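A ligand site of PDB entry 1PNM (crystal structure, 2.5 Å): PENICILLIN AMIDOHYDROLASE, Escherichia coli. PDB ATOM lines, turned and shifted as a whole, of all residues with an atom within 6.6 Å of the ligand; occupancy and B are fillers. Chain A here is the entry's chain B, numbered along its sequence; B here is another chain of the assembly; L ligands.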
ATOM      1  N   SER A   1     -32.102  22.913 -10.970  1.00  0.00           N
ATOM      2  CA  SER A   1     -31.350  24.088 -10.632  1.00  0.00           C
ATOM      3  C   SER A   1     -31.683  25.048 -11.766  1.00  0.00           C
ATOM      4  O   SER A   1     -31.424  24.711 -12.928  1.00  0.00           O
ATOM      5  CB  SER A   1     -29.837  23.987 -10.581  1.00  0.00           C
ATOM      6  OG  SER A   1     -29.417  23.310  -9.422  1.00  0.00           O
ATOM      7  N   ASN A   2     -32.186  26.160 -11.251  1.00  0.00           N
ATOM      8  CA  ASN A   2     -32.539  27.210 -12.271  1.00  0.00           C
ATOM      9  C   ASN A   2     -31.646  28.472 -12.224  1.00  0.00           C
ATOM     10  O   ASN A   2     -30.910  28.810 -11.280  1.00  0.00           O
ATOM     11  CB  ASN A   2     -34.015  27.548 -12.260  1.00  0.00           C
ATOM     12  CG  ASN A   2     -34.658  27.910 -10.943  1.00  0.00           C
ATOM     13  OD1 ASN A   2     -35.823  27.569 -10.638  1.00  0.00           O
ATOM     14  ND2 ASN A   2     -33.876  28.642 -10.151  1.00  0.00           N
ATOM     15  N   ASN A  20     -29.876  33.200  -9.714  1.00  0.00           N
ATOM     16  CA  ASN A  20     -29.496  31.783  -9.643  1.00  0.00           C
ATOM     17  C   ASN A  20     -30.164  31.131  -8.436  1.00  0.00           C
ATOM     18  O   ASN A  20     -30.130  31.689  -7.349  1.00  0.00           O
ATOM     19  CB  ASN A  20     -27.972  31.744  -9.585  1.00  0.00           C
ATOM     20  CG  ASN A  20     -27.276  30.503 -10.046  1.00  0.00           C
ATOM     21  OD1 ASN A  20     -26.025  30.526 -10.062  1.00  0.00           O
ATOM     22  ND2 ASN A  20     -27.959  29.418 -10.465  1.00  0.00           N
ATOM     23  N   GLY A  21     -30.642  29.917  -8.636  1.00  0.00           N
ATOM     24  CA  GLY A  21     -31.271  29.044  -7.649  1.00  0.00           C
ATOM     25  C   GLY A  21     -30.828  27.582  -7.877  1.00  0.00           C
ATOM     26  O   GLY A  21     -31.586  26.683  -8.321  1.00  0.00           O
ATOM     27  N   PRO A  22     -29.602  27.348  -7.385  1.00  0.00           N
ATOM     28  CA  PRO A  22     -29.000  25.994  -7.456  1.00  0.00           C
ATOM     29  C   PRO A  22     -29.812  25.133  -6.501  1.00  0.00           C
ATOM     30  O   PRO A  22     -30.104  25.558  -5.364  1.00  0.00           O
ATOM     31  CB  PRO A  22     -27.576  26.180  -7.037  1.00  0.00           C
ATOM     32  CG  PRO A  22     -27.665  27.362  -6.072  1.00  0.00           C
ATOM     33  CD  PRO A  22     -28.635  28.286  -6.776  1.00  0.00           C
ATOM     34  N   GLN A  23     -30.195  23.939  -6.937  1.00  0.00           N
ATOM     35  CA  GLN A  23     -31.069  23.026  -6.164  1.00  0.00           C
ATOM     36  C   GLN A  23     -30.343  21.773  -5.757  1.00  0.00           C
ATOM     37  O   GLN A  23     -30.089  20.857  -6.584  1.00  0.00           O
ATOM     38  CB  GLN A  23     -32.361  22.666  -6.939  1.00  0.00           C
ATOM     39  CG  GLN A  23     -33.298  23.857  -7.082  1.00  0.00           C
ATOM     40  CD  GLN A  23     -34.612  23.620  -7.781  1.00  0.00           C
ATOM     41  OE1 GLN A  23     -34.639  23.376  -8.988  1.00  0.00           O
ATOM     42  NE2 GLN A  23     -35.768  23.660  -7.077  1.00  0.00           N
ATOM     43  N   PHE A  24     -30.011  21.714  -4.463  1.00  0.00           N
ATOM     44  CA  PHE A  24     -29.233  20.561  -4.001  1.00  0.00           C
ATOM     45  C   PHE A  24     -29.894  19.842  -2.843  1.00  0.00           C
ATOM     46  O   PHE A  24     -29.244  18.901  -2.330  1.00  0.00           O
ATOM     47  CB  PHE A  24     -27.843  21.060  -3.578  1.00  0.00           C
ATOM     48  CG  PHE A  24     -26.927  21.870  -4.429  1.00  0.00           C
ATOM     49  CD1 PHE A  24     -26.114  21.400  -5.465  1.00  0.00           C
ATOM     50  CD2 PHE A  24     -26.870  23.243  -4.121  1.00  0.00           C
ATOM     51  CE1 PHE A  24     -25.256  22.278  -6.147  1.00  0.00           C
ATOM     52  CE2 PHE A  24     -26.023  24.130  -4.794  1.00  0.00           C
ATOM     53  CZ  PHE A  24     -25.218  23.648  -5.827  1.00  0.00           C
ATOM     54  N   PRO A  49     -20.768  25.775  -2.506  1.00  0.00           N
ATOM     55  CA  PRO A  49     -21.008  24.497  -1.843  1.00  0.00           C
ATOM     56  C   PRO A  49     -19.808  23.934  -1.134  1.00  0.00           C
ATOM     57  O   PRO A  49     -18.672  23.973  -1.638  1.00  0.00           O
ATOM     58  CB  PRO A  49     -21.438  23.533  -2.951  1.00  0.00           C
ATOM     59  CG  PRO A  49     -21.685  24.373  -4.167  1.00  0.00           C
ATOM     60  CD  PRO A  49     -21.004  25.731  -3.957  1.00  0.00           C
ATOM     61  N   VAL A  56     -18.697  29.060  -6.595  1.00  0.00           N
ATOM     62  CA  VAL A  56     -19.604  28.625  -7.712  1.00  0.00           C
ATOM     63  C   VAL A  56     -20.533  29.778  -8.021  1.00  0.00           C
ATOM     64  O   VAL A  56     -20.988  30.039  -9.162  1.00  0.00           O
ATOM     65  CB  VAL A  56     -20.234  27.255  -7.401  1.00  0.00           C
ATOM     66  CG1 VAL A  56     -21.202  26.809  -8.501  1.00  0.00           C
ATOM     67  CG2 VAL A  56     -19.242  26.145  -7.107  1.00  0.00           C
ATOM     68  N   PHE A  57     -20.973  30.544  -6.986  1.00  0.00           N
ATOM     69  CA  PHE A  57     -21.899  31.694  -7.139  1.00  0.00           C
ATOM     70  C   PHE A  57     -21.318  33.001  -6.568  1.00  0.00           C
ATOM     71  O   PHE A  57     -21.015  33.041  -5.344  1.00  0.00           O
ATOM     72  CB  PHE A  57     -23.302  31.406  -6.540  1.00  0.00           C
ATOM     73  CG  PHE A  57     -23.733  29.955  -6.588  1.00  0.00           C
ATOM     74  CD1 PHE A  57     -24.147  29.385  -7.816  1.00  0.00           C
ATOM     75  CD2 PHE A  57     -23.560  29.142  -5.464  1.00  0.00           C
ATOM     76  CE1 PHE A  57     -24.441  28.035  -7.880  1.00  0.00           C
ATOM     77  CE2 PHE A  57     -23.870  27.782  -5.505  1.00  0.00           C
ATOM     78  CZ  PHE A  57     -24.272  27.250  -6.722  1.00  0.00           C
ATOM     79  N   SER A  67     -23.940  28.690 -12.125  1.00  0.00           N
ATOM     80  CA  SER A  67     -24.043  27.347 -12.646  1.00  0.00           C
ATOM     81  C   SER A  67     -25.342  26.590 -12.507  1.00  0.00           C
ATOM     82  O   SER A  67     -26.162  26.940 -11.605  1.00  0.00           O
ATOM     83  CB  SER A  67     -23.059  26.609 -11.672  1.00  0.00           C
ATOM     84  OG  SER A  67     -21.905  26.203 -12.377  1.00  0.00           O
ATOM     85  N   THR A  68     -25.651  25.561 -13.274  1.00  0.00           N
ATOM     86  CA  THR A  68     -26.808  24.650 -13.190  1.00  0.00           C
ATOM     87  C   THR A  68     -26.294  23.301 -13.694  1.00  0.00           C
ATOM     88  O   THR A  68     -25.383  23.308 -14.539  1.00  0.00           O
ATOM     89  CB  THR A  68     -28.148  25.045 -13.862  1.00  0.00           C
ATOM     90  OG1 THR A  68     -27.953  25.021 -15.311  1.00  0.00           O
ATOM     91  CG2 THR A  68     -28.742  26.427 -13.502  1.00  0.00           C
ATOM     92  N   ALA A  69     -26.720  22.191 -13.182  1.00  0.00           N
ATOM     93  CA  ALA A  69     -26.257  20.827 -13.600  1.00  0.00           C
ATOM     94  C   ALA A  69     -26.465  20.679 -15.100  1.00  0.00           C
ATOM     95  O   ALA A  69     -27.516  21.123 -15.612  1.00  0.00           O
ATOM     96  CB  ALA A  69     -26.927  19.867 -12.652  1.00  0.00           C
ATOM     97  N   GLY A  70     -25.523  20.175 -15.879  1.00  0.00           N
ATOM     98  CA  GLY A  70     -25.583  20.050 -17.318  1.00  0.00           C
ATOM     99  C   GLY A  70     -26.384  18.904 -17.910  1.00  0.00           C
ATOM    100  O   GLY A  70     -27.123  19.092 -18.893  1.00  0.00           O
ATOM    101  N   PHE A  71     -26.231  17.710 -17.375  1.00  0.00           N
ATOM    102  CA  PHE A  71     -26.824  16.430 -17.736  1.00  0.00           C
ATOM    103  C   PHE A  71     -26.493  15.939 -19.145  1.00  0.00           C
ATOM    104  O   PHE A  71     -27.368  15.279 -19.766  1.00  0.00           O
ATOM    105  CB  PHE A  71     -28.363  16.345 -17.495  1.00  0.00           C
ATOM    106  CG  PHE A  71     -28.627  16.298 -16.021  1.00  0.00           C
ATOM    107  CD1 PHE A  71     -28.518  15.059 -15.367  1.00  0.00           C
ATOM    108  CD2 PHE A  71     -28.961  17.457 -15.302  1.00  0.00           C
ATOM    109  CE1 PHE A  71     -28.762  14.953 -13.981  1.00  0.00           C
ATOM    110  CE2 PHE A  71     -29.209  17.373 -13.935  1.00  0.00           C
ATOM    111  CZ  PHE A  71     -29.085  16.143 -13.280  1.00  0.00           C
ATOM    112  N   TRP A 154     -12.560  26.482 -11.799  1.00  0.00           N
ATOM    113  CA  TRP A 154     -13.582  27.102 -10.977  1.00  0.00           C
ATOM    114  C   TRP A 154     -13.010  28.232 -10.072  1.00  0.00           C
ATOM    115  O   TRP A 154     -13.736  29.203  -9.760  1.00  0.00           O
ATOM    116  CB  TRP A 154     -14.382  26.089 -10.104  1.00  0.00           C
ATOM    117  CG  TRP A 154     -15.857  26.185 -10.349  1.00  0.00           C
ATOM    118  CD1 TRP A 154     -16.662  27.282 -10.336  1.00  0.00           C
ATOM    119  CD2 TRP A 154     -16.689  25.071 -10.691  1.00  0.00           C
ATOM    120  NE1 TRP A 154     -17.937  26.934 -10.667  1.00  0.00           N
ATOM    121  CE2 TRP A 154     -17.995  25.574 -10.892  1.00  0.00           C
ATOM    122  CE3 TRP A 154     -16.460  23.698 -10.850  1.00  0.00           C
ATOM    123  CZ2 TRP A 154     -19.051  24.732 -11.225  1.00  0.00           C
ATOM    124  CZ3 TRP A 154     -17.497  22.859 -11.195  1.00  0.00           C
ATOM    125  CH2 TRP A 154     -18.774  23.378 -11.369  1.00  0.00           C
ATOM    126  N   THR A 176     -19.885  17.861 -16.502  1.00  0.00           N
ATOM    127  CA  THR A 176     -21.046  18.319 -17.304  1.00  0.00           C
ATOM    128  C   THR A 176     -21.852  19.344 -16.534  1.00  0.00           C
ATOM    129  O   THR A 176     -22.712  18.994 -15.682  1.00  0.00           O
ATOM    130  CB  THR A 176     -21.929  17.110 -17.839  1.00  0.00           C
ATOM    131  OG1 THR A 176     -22.947  17.824 -18.628  1.00  0.00           O
ATOM    132  CG2 THR A 176     -22.644  16.157 -16.868  1.00  0.00           C
ATOM    133  N   ILE A 177     -21.561  20.627 -16.707  1.00  0.00           N
ATOM    134  CA  ILE A 177     -22.149  21.742 -15.978  1.00  0.00           C
ATOM    135  C   ILE A 177     -22.443  22.942 -16.868  1.00  0.00           C
ATOM    136  O   ILE A 177     -21.577  23.327 -17.700  1.00  0.00           O
ATOM    137  CB  ILE A 177     -21.166  22.282 -14.802  1.00  0.00           C
ATOM    138  CG1 ILE A 177     -20.528  21.262 -13.840  1.00  0.00           C
ATOM    139  CG2 ILE A 177     -21.818  23.398 -13.949  1.00  0.00           C
ATOM    140  CD1 ILE A 177     -21.433  20.439 -12.884  1.00  0.00           C
ATOM    141  N   ASN A 178     -23.562  23.626 -16.693  1.00  0.00           N
ATOM    142  CA  ASN A 178     -23.853  24.847 -17.430  1.00  0.00           C
ATOM    143  C   ASN A 178     -23.203  26.024 -16.659  1.00  0.00           C
ATOM    144  O   ASN A 178     -23.457  26.127 -15.424  1.00  0.00           O
ATOM    145  CB  ASN A 178     -25.367  25.054 -17.527  1.00  0.00           C
ATOM    146  CG  ASN A 178     -26.027  23.961 -18.347  1.00  0.00           C
ATOM    147  OD1 ASN A 178     -25.602  23.716 -19.496  1.00  0.00           O
ATOM    148  ND2 ASN A 178     -27.037  23.240 -17.848  1.00  0.00           N
ATOM    149  N   ASN A 239     -32.594  28.562 -17.840  1.00  0.00           N
ATOM    150  CA  ASN A 239     -32.288  27.119 -17.742  1.00  0.00           C
ATOM    151  C   ASN A 239     -32.857  26.503 -16.462  1.00  0.00           C
ATOM    152  O   ASN A 239     -32.827  27.158 -15.403  1.00  0.00           O
ATOM    153  CB  ASN A 239     -30.763  26.893 -17.891  1.00  0.00           C
ATOM    154  CG  ASN A 239     -30.381  25.416 -17.922  1.00  0.00           C
ATOM    155  OD1 ASN A 239     -30.242  24.717 -16.916  1.00  0.00           O
ATOM    156  ND2 ASN A 239     -30.185  24.876 -19.136  1.00  0.00           N
ATOM    157  N   ASN A 241     -32.327  22.917 -16.024  1.00  0.00           N
ATOM    158  CA  ASN A 241     -31.724  21.620 -16.353  1.00  0.00           C
ATOM    159  C   ASN A 241     -32.318  20.968 -17.652  1.00  0.00           C
ATOM    160  O   ASN A 241     -32.394  19.742 -17.822  1.00  0.00           O
ATOM    161  CB  ASN A 241     -31.724  20.574 -15.256  1.00  0.00           C
ATOM    162  CG  ASN A 241     -31.259  20.958 -13.889  1.00  0.00           C
ATOM    163  OD1 ASN A 241     -32.020  20.821 -12.930  1.00  0.00           O
ATOM    164  ND2 ASN A 241     -30.068  21.502 -13.767  1.00  0.00           N
ATOM    165  N   ARG A 263     -40.055  21.821 -17.645  1.00  0.00           N
ATOM    166  CA  ARG A 263     -40.300  22.858 -16.618  1.00  0.00           C
ATOM    167  C   ARG A 263     -39.638  24.174 -16.943  1.00  0.00           C
ATOM    168  O   ARG A 263     -40.203  25.195 -16.432  1.00  0.00           O
ATOM    169  CB  ARG A 263     -39.925  22.430 -15.204  1.00  0.00           C
ATOM    170  CG  ARG A 263     -38.467  22.029 -15.047  1.00  0.00           C
ATOM    171  CD  ARG A 263     -38.151  21.730 -13.621  1.00  0.00           C
ATOM    172  NE  ARG A 263     -36.742  21.438 -13.440  1.00  0.00           N
ATOM    173  CZ  ARG A 263     -36.256  20.776 -12.395  1.00  0.00           C
ATOM    174  NH1 ARG A 263     -36.978  20.287 -11.389  1.00  0.00           N
ATOM    175  NH2 ARG A 263     -34.916  20.596 -12.357  1.00  0.00           N
ATOM    176  N   SER A 386     -35.953  19.329  -5.865  1.00  0.00           N
ATOM    177  CA  SER A 386     -36.931  19.947  -6.744  1.00  0.00           C
ATOM    178  C   SER A 386     -38.028  18.990  -7.257  1.00  0.00           C
ATOM    179  O   SER A 386     -38.002  17.764  -7.393  1.00  0.00           O
ATOM    180  CB  SER A 386     -36.194  20.492  -7.987  1.00  0.00           C
ATOM    181  OG  SER A 386     -35.861  19.461  -8.923  1.00  0.00           O
ATOM    182  N   MET B 142     -19.258  17.054  -6.152  1.00  0.00           N
ATOM    183  CA  MET B 142     -19.494  17.772  -7.399  1.00  0.00           C
ATOM    184  C   MET B 142     -19.303  16.766  -8.554  1.00  0.00           C
ATOM    185  O   MET B 142     -20.221  16.607  -9.369  1.00  0.00           O
ATOM    186  CB  MET B 142     -18.662  19.031  -7.564  1.00  0.00           C
ATOM    187  CG  MET B 142     -19.051  19.817  -8.786  1.00  0.00           C
ATOM    188  SD  MET B 142     -20.746  20.462  -8.747  1.00  0.00           S
ATOM    189  CE  MET B 142     -20.534  22.134  -8.062  1.00  0.00           C
ATOM    190  N   PHE B 146     -23.045  15.217  -9.340  1.00  0.00           N
ATOM    191  CA  PHE B 146     -23.643  15.726 -10.579  1.00  0.00           C
ATOM    192  C   PHE B 146     -22.970  15.406 -11.921  1.00  0.00           C
ATOM    193  O   PHE B 146     -23.446  15.982 -12.917  1.00  0.00           O
ATOM    194  CB  PHE B 146     -23.864  17.265 -10.434  1.00  0.00           C
ATOM    195  CG  PHE B 146     -24.705  17.700  -9.278  1.00  0.00           C
ATOM    196  CD1 PHE B 146     -26.091  17.436  -9.393  1.00  0.00           C
ATOM    197  CD2 PHE B 146     -24.195  18.269  -8.099  1.00  0.00           C
ATOM    198  CE1 PHE B 146     -26.997  17.742  -8.362  1.00  0.00           C
ATOM    199  CE2 PHE B 146     -25.087  18.574  -7.071  1.00  0.00           C
ATOM    200  CZ  PHE B 146     -26.473  18.311  -7.186  1.00  0.00           C
HETATM  201  C1  LIG L   1     -27.574  21.817  -8.692  1.00  0.00           C
HETATM  202  S1  LIG L   1     -28.887  21.907 -10.002  1.00  0.00           S
HETATM  203  C2  LIG L   1     -26.196  22.161  -9.196  1.00  0.00           C
HETATM  204  C3  LIG L   1     -25.811  23.475  -9.199  1.00  0.00           C
HETATM  205  C4  LIG L   1     -24.572  23.767  -9.757  1.00  0.00           C
HETATM  206  C5  LIG L   1     -23.842  22.717 -10.307  1.00  0.00           C
HETATM  207  C6  LIG L   1     -24.254  21.381 -10.319  1.00  0.00           C
HETATM  208  C7  LIG L   1     -25.472  21.132  -9.741  1.00  0.00           C
HETATM  209  O1  LIG L   1     -28.267  21.995 -11.339  1.00  0.00           O
HETATM  210  O2  LIG L   1     -29.463  20.493  -9.904  1.00  0.00           O
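OG of Ser 67 sits close to O of Asn 178 (3.4 Å). O of Ala 69 is in hydrogen-bond range of ND2 of Asn 241, at 3.2 Å. The side-chain amide oxygen (OD1) of Asn 239 sits at hydrogen-bond distance from the side-chain hydroxyl (OG1) of Thr 68. The backbone carbonyl oxygen (O) of Ala 69 lies within hydrogen-bond range of the side-chain amide nitrogen (ND2) of Asn 178 (3.1 Å). The side-chain amide oxygen (OD1) of Asn 239 sits at hydrogen-bond distance from the backbone NH (N) of Asn 241. The side-chain hydroxyl (OG) of Ser 1 is in hydrogen-bond range of the backbone NH (N) of Gln 23. O of Thr 68 sits at hydrogen-bond distance from N of Asn 178. The side-chain amide nitrogen of Asn 20 lies within hydrogen-bond range of the backbone carbonyl oxygen of Ser 67, 3.3 Å away.
An oxygen (O1) of the ligand lies within hydrogen-bond range of the side-chain amide nitrogen (ND2) of Asn 241 (3.1 Å). The backbone NH (N) of Ala 69 is in hydrogen-bond range of an oxygen (O1) of the ligand. OG of Ser 1 is bonded to S1 of the ligand (1.6 Å).
O of Gln 23 sits close to O2 of the ligand (3.4 Å). Merely in contact with the ligand: Pro 22 (3.9 Å), Phe 24 (3.2 Å), Ser 67 (3.7 Å), Thr 68 (3.3 Å), Ile 177 (3.9 Å), Met 142 of chain B (3.95 Å) and Phe 146 of chain B (3.5 Å). Hydrophobic or aromatic side chains within 4 Å of the ligand: Pro 22, Phe 24, Ala 69, Ile 177, Met 142 of chain B and Phe 146 of chain B. Of the 25 residues printed, 11 come within 4 Å of the ligand. The nearest printed residue that does not touch the ligand is Phe 57 (4.6 Å).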
